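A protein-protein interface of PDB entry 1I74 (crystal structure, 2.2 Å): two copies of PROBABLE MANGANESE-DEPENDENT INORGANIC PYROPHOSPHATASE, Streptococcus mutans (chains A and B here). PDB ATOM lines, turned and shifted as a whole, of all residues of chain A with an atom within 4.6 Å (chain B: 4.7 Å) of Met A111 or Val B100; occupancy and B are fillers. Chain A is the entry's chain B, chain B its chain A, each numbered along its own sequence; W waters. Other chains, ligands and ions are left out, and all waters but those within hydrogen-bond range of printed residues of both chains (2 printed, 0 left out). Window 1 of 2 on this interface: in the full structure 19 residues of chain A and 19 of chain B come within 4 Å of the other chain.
The side-chain amide nitrogen (ND2) of Asn B77 sits at hydrogen-bond distance from the backbone carbonyl oxygen (O) of Arg B99, at 3.0 Å.
OD1 of Asn B77 lies within hydrogen-bond range of N of Ala B101 (3.3 Å).
O of Tyr A110 sits at hydrogen-bond distance from N of Val A94 (3.0 Å).
O of Val A94 is in hydrogen-bond range of N of Arg A112, 2.7 Å away.
NH1 of Arg A112 sits at hydrogen-bond distance from OH of Tyr A110.
Of the 9 printed residues of chain A, 8 touch a printed residue of chain B.
Printed residues of chain A that touch a printed residue of chain B: Phe A103, Glu A104, Thr A105, Leu A109, Tyr A110, Met A111, Arg A112 and Leu A113.
Hydrophobic or aromatic side chains of chain A that line the printed part of chain B: Phe A103, Tyr A110, Met A111 and Leu A113.
Of the 9 printed residues of chain B, 6 touch a printed residue of chain A.
Hydrophobic or aromatic side chains of chain B within 4 Å of the printed part of chain A: Val B100, Ala B101, Met B111 and Leu B113.
Printed residues of chain B within 4 Å of Tyr A110: Arg B112 and Leu B113.
Of chain B, only Val B100 (3.8 Å), Met B111 (3.1 Å), Arg B112 (3.3 Å) and Leu B113 (2.8 Å) come within 4 Å of Met A111.
Printed residues of chain A within 4 Å of Arg B99: Thr A105 (2.9 Å).
Val B100 touches just these residues of chain A: Phe A103 (3.9 Å), Glu A104 (3.4 Å), Thr A105 (2.9 Å) and Met A111 (3.8 Å).
The nearest printed residue of chain B that does not touch Met A111 is His B98 (6.9 Å).
The nearest residue of chain A that does not touch Val B100 is Leu A109 (4.3 Å).
Val B100 touches Phe A103.
Glu A104 touches Val B100.
Glu A104 touches Ala B101 (CG to CB, 3.8 Å).
Tyr A110 touches Arg B112.
O of Leu B113 touches CA of Tyr A110, at 3.1 Å.
Val B100 touches Met A111 (CG2 to SD, 3.8 Å).
CA of Arg B112 touches O of Met A111, 3.3 Å away.
Met B111 touches Arg A112 (O to CA, 3.3 Å).
The guanidinium group (NH1) of Arg B99 sits at hydrogen-bond distance from the backbone carbonyl oxygen (O) of Thr A105 (2.9 Å).
N of Thr A105 sits at hydrogen-bond distance from O of Val B100 (2.9 Å).
N of Met B111 is in hydrogen-bond range of O of Leu A113.
The backbone NH (N) of Met A111 sits at hydrogen-bond distance from the backbone carbonyl oxygen (O) of Leu B113.
The backbone carbonyl oxygen of Leu B113 sits close to the backbone carbonyl oxygen of Leu A109.
O of Met B111 sits close to O of Met A111, at 3.1 Å.
NH1 of Arg A112 sits close to NH1 of Arg B112, at 3.4 Å.
Met B111 touches its own counterpart, Met A111.
Met A111 touches Arg B112, and with the chains exchanged Arg A112 touches Met B111.
Met A111 touches Leu B113, and with the chains exchanged Leu A113 touches Met B111.
Arg A112 touches its own counterpart, Arg B112.
Positions printed for both chains: 103, 111, 112 and 113.
Of the 15 pairs that touch across the chains among the printed residues, 6 have their exchanged pair printed and touching as well.
Water W1 bridges OH of Tyr A110 (2.5 Å) and NH2 of Arg B112 (3.5 Å).
Water W2 lies within hydrogen-bond range of the backbone carbonyl oxygen (O) of Leu A109 and the backbone carbonyl oxygen (O) of His B98.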
ATOM      1  N   VAL A  94       5.244 -24.610 -12.667  1.00  0.00           N
ATOM      2  CA  VAL A  94       5.050 -23.391 -13.429  1.00  0.00           C
ATOM      3  C   VAL A  94       6.368 -22.641 -13.572  1.00  0.00           C
ATOM      4  O   VAL A  94       7.076 -22.414 -12.586  1.00  0.00           O
ATOM      5  CB  VAL A  94       4.036 -22.437 -12.771  1.00  0.00           C
ATOM      6  CG1 VAL A  94       3.840 -21.221 -13.659  1.00  0.00           C
ATOM      7  CG2 VAL A  94       2.720 -23.148 -12.538  1.00  0.00           C
ATOM      8  N   PHE A 103      -4.951 -17.778 -10.675  1.00  0.00           N
ATOM      9  CA  PHE A 103      -4.177 -19.003 -10.584  1.00  0.00           C
ATOM     10  C   PHE A 103      -4.308 -19.562  -9.175  1.00  0.00           C
ATOM     11  O   PHE A 103      -4.123 -18.838  -8.204  1.00  0.00           O
ATOM     12  CB  PHE A 103      -2.706 -18.719 -10.871  1.00  0.00           C
ATOM     13  CG  PHE A 103      -1.816 -19.905 -10.670  1.00  0.00           C
ATOM     14  CD1 PHE A 103      -1.724 -20.897 -11.641  1.00  0.00           C
ATOM     15  CD2 PHE A 103      -1.106 -20.059  -9.490  1.00  0.00           C
ATOM     16  CE1 PHE A 103      -0.942 -22.026 -11.441  1.00  0.00           C
ATOM     17  CE2 PHE A 103      -0.317 -21.188  -9.277  1.00  0.00           C
ATOM     18  CZ  PHE A 103      -0.239 -22.176 -10.259  1.00  0.00           C
ATOM     19  N   GLU A 104      -4.621 -20.846  -9.066  1.00  0.00           N
ATOM     20  CA  GLU A 104      -4.765 -21.475  -7.759  1.00  0.00           C
ATOM     21  C   GLU A 104      -4.515 -22.973  -7.840  1.00  0.00           C
ATOM     22  O   GLU A 104      -4.859 -23.619  -8.822  1.00  0.00           O
ATOM     23  CB  GLU A 104      -6.170 -21.231  -7.207  1.00  0.00           C
ATOM     24  CG  GLU A 104      -6.400 -21.831  -5.832  1.00  0.00           C
ATOM     25  CD  GLU A 104      -7.823 -21.615  -5.319  1.00  0.00           C
ATOM     26  OE1 GLU A 104      -8.334 -20.482  -5.443  1.00  0.00           O
ATOM     27  OE2 GLU A 104      -8.423 -22.578  -4.784  1.00  0.00           O
ATOM     28  N   THR A 105      -3.916 -23.527  -6.796  1.00  0.00           N
ATOM     29  CA  THR A 105      -3.655 -24.957  -6.759  1.00  0.00           C
ATOM     30  C   THR A 105      -4.176 -25.521  -5.451  1.00  0.00           C
ATOM     31  O   THR A 105      -4.189 -24.844  -4.427  1.00  0.00           O
ATOM     32  CB  THR A 105      -2.148 -25.263  -6.856  1.00  0.00           C
ATOM     33  OG1 THR A 105      -1.505 -24.909  -5.623  1.00  0.00           O
ATOM     34  CG2 THR A 105      -1.524 -24.477  -8.008  1.00  0.00           C
ATOM     35  N   LEU A 109       3.282 -27.202  -5.117  1.00  0.00           N
ATOM     36  CA  LEU A 109       3.836 -27.468  -6.440  1.00  0.00           C
ATOM     37  C   LEU A 109       5.181 -26.782  -6.618  1.00  0.00           C
ATOM     38  O   LEU A 109       5.622 -26.018  -5.760  1.00  0.00           O
ATOM     39  CB  LEU A 109       2.890 -26.959  -7.532  1.00  0.00           C
ATOM     40  CG  LEU A 109       2.826 -25.432  -7.683  1.00  0.00           C
ATOM     41  CD1 LEU A 109       2.069 -25.045  -8.937  1.00  0.00           C
ATOM     42  CD2 LEU A 109       2.158 -24.841  -6.465  1.00  0.00           C
ATOM     43  N   TYR A 110       5.828 -27.061  -7.744  1.00  0.00           N
ATOM     44  CA  TYR A 110       7.096 -26.434  -8.058  1.00  0.00           C
ATOM     45  C   TYR A 110       6.791 -25.205  -8.903  1.00  0.00           C
ATOM     46  O   TYR A 110       6.101 -25.293  -9.915  1.00  0.00           O
ATOM     47  CB  TYR A 110       8.014 -27.371  -8.856  1.00  0.00           C
ATOM     48  CG  TYR A 110       9.366 -26.735  -9.159  1.00  0.00           C
ATOM     49  CD1 TYR A 110      10.302 -26.533  -8.140  1.00  0.00           C
ATOM     50  CD2 TYR A 110       9.669 -26.234 -10.439  1.00  0.00           C
ATOM     51  CE1 TYR A 110      11.502 -25.835  -8.377  1.00  0.00           C
ATOM     52  CE2 TYR A 110      10.874 -25.532 -10.689  1.00  0.00           C
ATOM     53  CZ  TYR A 110      11.778 -25.334  -9.649  1.00  0.00           C
ATOM     54  OH  TYR A 110      12.938 -24.608  -9.839  1.00  0.00           O
ATOM     55  N   MET A 111       7.283 -24.054  -8.471  1.00  0.00           N
ATOM     56  CA  MET A 111       7.088 -22.836  -9.224  1.00  0.00           C
ATOM     57  C   MET A 111       8.391 -22.082  -9.319  1.00  0.00           C
ATOM     58  O   MET A 111       9.094 -21.909  -8.331  1.00  0.00           O
ATOM     59  CB  MET A 111       6.044 -21.942  -8.575  1.00  0.00           C
ATOM     60  CG  MET A 111       4.623 -22.408  -8.773  1.00  0.00           C
ATOM     61  SD  MET A 111       3.457 -20.959  -8.252  1.00  0.00           S
ATOM     62  CE  MET A 111       3.309 -20.003  -9.931  1.00  0.00           C
ATOM     63  N   ARG A 112       8.705 -21.632 -10.523  1.00  0.00           N
ATOM     64  CA  ARG A 112       9.918 -20.887 -10.766  1.00  0.00           C
ATOM     65  C   ARG A 112       9.560 -19.683 -11.624  1.00  0.00           C
ATOM     66  O   ARG A 112       9.479 -19.770 -12.849  1.00  0.00           O
ATOM     67  CB  ARG A 112      10.951 -21.777 -11.462  1.00  0.00           C
ATOM     68  CG  ARG A 112      12.302 -21.126 -11.697  1.00  0.00           C
ATOM     69  CD  ARG A 112      12.936 -20.592 -10.415  1.00  0.00           C
ATOM     70  NE  ARG A 112      14.272 -20.077 -10.686  1.00  0.00           N
ATOM     71  CZ  ARG A 112      15.365 -20.831 -10.764  1.00  0.00           C
ATOM     72  NH1 ARG A 112      15.285 -22.140 -10.575  1.00  0.00           N
ATOM     73  NH2 ARG A 112      16.531 -20.284 -11.064  1.00  0.00           N
ATOM     74  N   LEU A 113       9.302 -18.569 -10.956  1.00  0.00           N
ATOM     75  CA  LEU A 113       8.966 -17.331 -11.628  1.00  0.00           C
ATOM     76  C   LEU A 113      10.105 -16.355 -11.385  1.00  0.00           C
ATOM     77  O   LEU A 113      10.617 -16.254 -10.275  1.00  0.00           O
ATOM     78  CB  LEU A 113       7.678 -16.725 -11.058  1.00  0.00           C
ATOM     79  CG  LEU A 113       6.299 -17.387 -11.152  1.00  0.00           C
ATOM     80  CD1 LEU A 113       5.394 -16.479 -11.957  1.00  0.00           C
ATOM     81  CD2 LEU A 113       6.365 -18.774 -11.766  1.00  0.00           C
ATOM     82  N   ASN B  77       1.974 -17.739   1.112  1.00  0.00           N
ATOM     83  CA  ASN B  77       1.683 -16.864  -0.015  1.00  0.00           C
ATOM     84  C   ASN B  77       0.262 -16.323   0.098  1.00  0.00           C
ATOM     85  O   ASN B  77      -0.008 -15.204  -0.345  1.00  0.00           O
ATOM     86  CB  ASN B  77       1.900 -17.584  -1.355  1.00  0.00           C
ATOM     87  CG  ASN B  77       0.971 -18.765  -1.562  1.00  0.00           C
ATOM     88  OD1 ASN B  77      -0.080 -18.650  -2.196  1.00  0.00           O
ATOM     89  ND2 ASN B  77       1.362 -19.913  -1.033  1.00  0.00           N
ATOM     90  N   HIS B  98       3.895 -24.292   0.061  1.00  0.00           N
ATOM     91  CA  HIS B  98       2.471 -24.542   0.186  1.00  0.00           C
ATOM     92  C   HIS B  98       1.774 -24.370  -1.146  1.00  0.00           C
ATOM     93  O   HIS B  98       2.344 -23.840  -2.107  1.00  0.00           O
ATOM     94  CB  HIS B  98       1.824 -23.578   1.173  1.00  0.00           C
ATOM     95  CG  HIS B  98       2.337 -23.702   2.569  1.00  0.00           C
ATOM     96  ND1 HIS B  98       3.462 -23.042   3.010  1.00  0.00           N
ATOM     97  CD2 HIS B  98       1.874 -24.409   3.625  1.00  0.00           C
ATOM     98  CE1 HIS B  98       3.669 -23.332   4.279  1.00  0.00           C
ATOM     99  NE2 HIS B  98       2.720 -24.160   4.678  1.00  0.00           N
ATOM    100  N   ARG B  99       0.527 -24.815  -1.194  1.00  0.00           N
ATOM    101  CA  ARG B  99      -0.254 -24.650  -2.393  1.00  0.00           C
ATOM    102  C   ARG B  99      -0.426 -23.132  -2.555  1.00  0.00           C
ATOM    103  O   ARG B  99      -0.205 -22.368  -1.619  1.00  0.00           O
ATOM    104  CB  ARG B  99      -1.605 -25.370  -2.251  1.00  0.00           C
ATOM    105  CG  ARG B  99      -2.536 -24.887  -1.124  1.00  0.00           C
ATOM    106  CD  ARG B  99      -3.236 -23.575  -1.469  1.00  0.00           C
ATOM    107  NE  ARG B  99      -4.416 -23.325  -0.634  1.00  0.00           N
ATOM    108  CZ  ARG B  99      -5.654 -23.691  -0.959  1.00  0.00           C
ATOM    109  NH1 ARG B  99      -5.877 -24.323  -2.106  1.00  0.00           N
ATOM    110  NH2 ARG B  99      -6.672 -23.418  -0.148  1.00  0.00           N
ATOM    111  N   VAL B 100      -0.782 -22.692  -3.751  1.00  0.00           N
ATOM    112  CA  VAL B 100      -0.974 -21.274  -3.990  1.00  0.00           C
ATOM    113  C   VAL B 100      -2.457 -20.952  -4.071  1.00  0.00           C
ATOM    114  O   VAL B 100      -3.215 -21.663  -4.729  1.00  0.00           O
ATOM    115  CB  VAL B 100      -0.303 -20.831  -5.295  1.00  0.00           C
ATOM    116  CG1 VAL B 100      -0.733 -19.426  -5.634  1.00  0.00           C
ATOM    117  CG2 VAL B 100       1.206 -20.903  -5.154  1.00  0.00           C
ATOM    118  N   ALA B 101      -2.861 -19.883  -3.390  1.00  0.00           N
ATOM    119  CA  ALA B 101      -4.251 -19.444  -3.374  1.00  0.00           C
ATOM    120  C   ALA B 101      -4.330 -18.068  -2.725  1.00  0.00           C
ATOM    121  O   ALA B 101      -3.447 -17.691  -1.968  1.00  0.00           O
ATOM    122  CB  ALA B 101      -5.101 -20.438  -2.601  1.00  0.00           C
ATOM    123  N   PHE B 103      -3.607 -15.324  -3.671  1.00  0.00           N
ATOM    124  CA  PHE B 103      -2.355 -14.635  -3.897  1.00  0.00           C
ATOM    125  C   PHE B 103      -2.431 -13.987  -5.265  1.00  0.00           C
ATOM    126  O   PHE B 103      -2.889 -14.606  -6.224  1.00  0.00           O
ATOM    127  CB  PHE B 103      -1.192 -15.632  -3.859  1.00  0.00           C
ATOM    128  CG  PHE B 103       0.137 -15.014  -4.161  1.00  0.00           C
ATOM    129  CD1 PHE B 103       0.868 -14.393  -3.162  1.00  0.00           C
ATOM    130  CD2 PHE B 103       0.632 -15.004  -5.464  1.00  0.00           C
ATOM    131  CE1 PHE B 103       2.077 -13.766  -3.447  1.00  0.00           C
ATOM    132  CE2 PHE B 103       1.843 -14.380  -5.764  1.00  0.00           C
ATOM    133  CZ  PHE B 103       2.569 -13.757  -4.752  1.00  0.00           C
ATOM    134  N   MET B 111       9.739 -16.182  -7.774  1.00  0.00           N
ATOM    135  CA  MET B 111       9.010 -17.171  -7.011  1.00  0.00           C
ATOM    136  C   MET B 111       9.741 -18.485  -7.060  1.00  0.00           C
ATOM    137  O   MET B 111      10.099 -18.968  -8.126  1.00  0.00           O
ATOM    138  CB  MET B 111       7.603 -17.348  -7.578  1.00  0.00           C
ATOM    139  CG  MET B 111       6.493 -17.092  -6.589  1.00  0.00           C
ATOM    140  SD  MET B 111       4.738 -16.950  -7.442  1.00  0.00           S
ATOM    141  CE  MET B 111       4.695 -15.064  -7.626  1.00  0.00           C
ATOM    142  N   ARG B 112       9.979 -19.052  -5.892  1.00  0.00           N
ATOM    143  CA  ARG B 112      10.629 -20.339  -5.811  1.00  0.00           C
ATOM    144  C   ARG B 112       9.800 -21.188  -4.866  1.00  0.00           C
ATOM    145  O   ARG B 112       9.914 -21.076  -3.647  1.00  0.00           O
ATOM    146  CB  ARG B 112      12.062 -20.187  -5.303  1.00  0.00           C
ATOM    147  CG  ARG B 112      12.844 -21.496  -5.165  1.00  0.00           C
ATOM    148  CD  ARG B 112      13.000 -22.266  -6.486  1.00  0.00           C
ATOM    149  NE  ARG B 112      13.905 -23.402  -6.319  1.00  0.00           N
ATOM    150  CZ  ARG B 112      15.191 -23.405  -6.676  1.00  0.00           C
ATOM    151  NH1 ARG B 112      15.734 -22.336  -7.242  1.00  0.00           N
ATOM    152  NH2 ARG B 112      15.944 -24.467  -6.431  1.00  0.00           N
ATOM    153  N   LEU B 113       8.923 -22.002  -5.437  1.00  0.00           N
ATOM    154  CA  LEU B 113       8.094 -22.884  -4.639  1.00  0.00           C
ATOM    155  C   LEU B 113       8.483 -24.306  -4.977  1.00  0.00           C
ATOM    156  O   LEU B 113       8.730 -24.628  -6.137  1.00  0.00           O
ATOM    157  CB  LEU B 113       6.604 -22.701  -4.938  1.00  0.00           C
ATOM    158  CG  LEU B 113       5.913 -21.337  -4.852  1.00  0.00           C
ATOM    159  CD1 LEU B 113       4.477 -21.588  -4.395  1.00  0.00           C
ATOM    160  CD2 LEU B 113       6.612 -20.389  -3.902  1.00  0.00           C
HETATM  161  O   HOH W   1      14.789 -26.153  -9.231  1.00  0.00           O
HETATM  162  O   HOH W   2       4.552 -25.457  -3.147  1.00  0.00           O
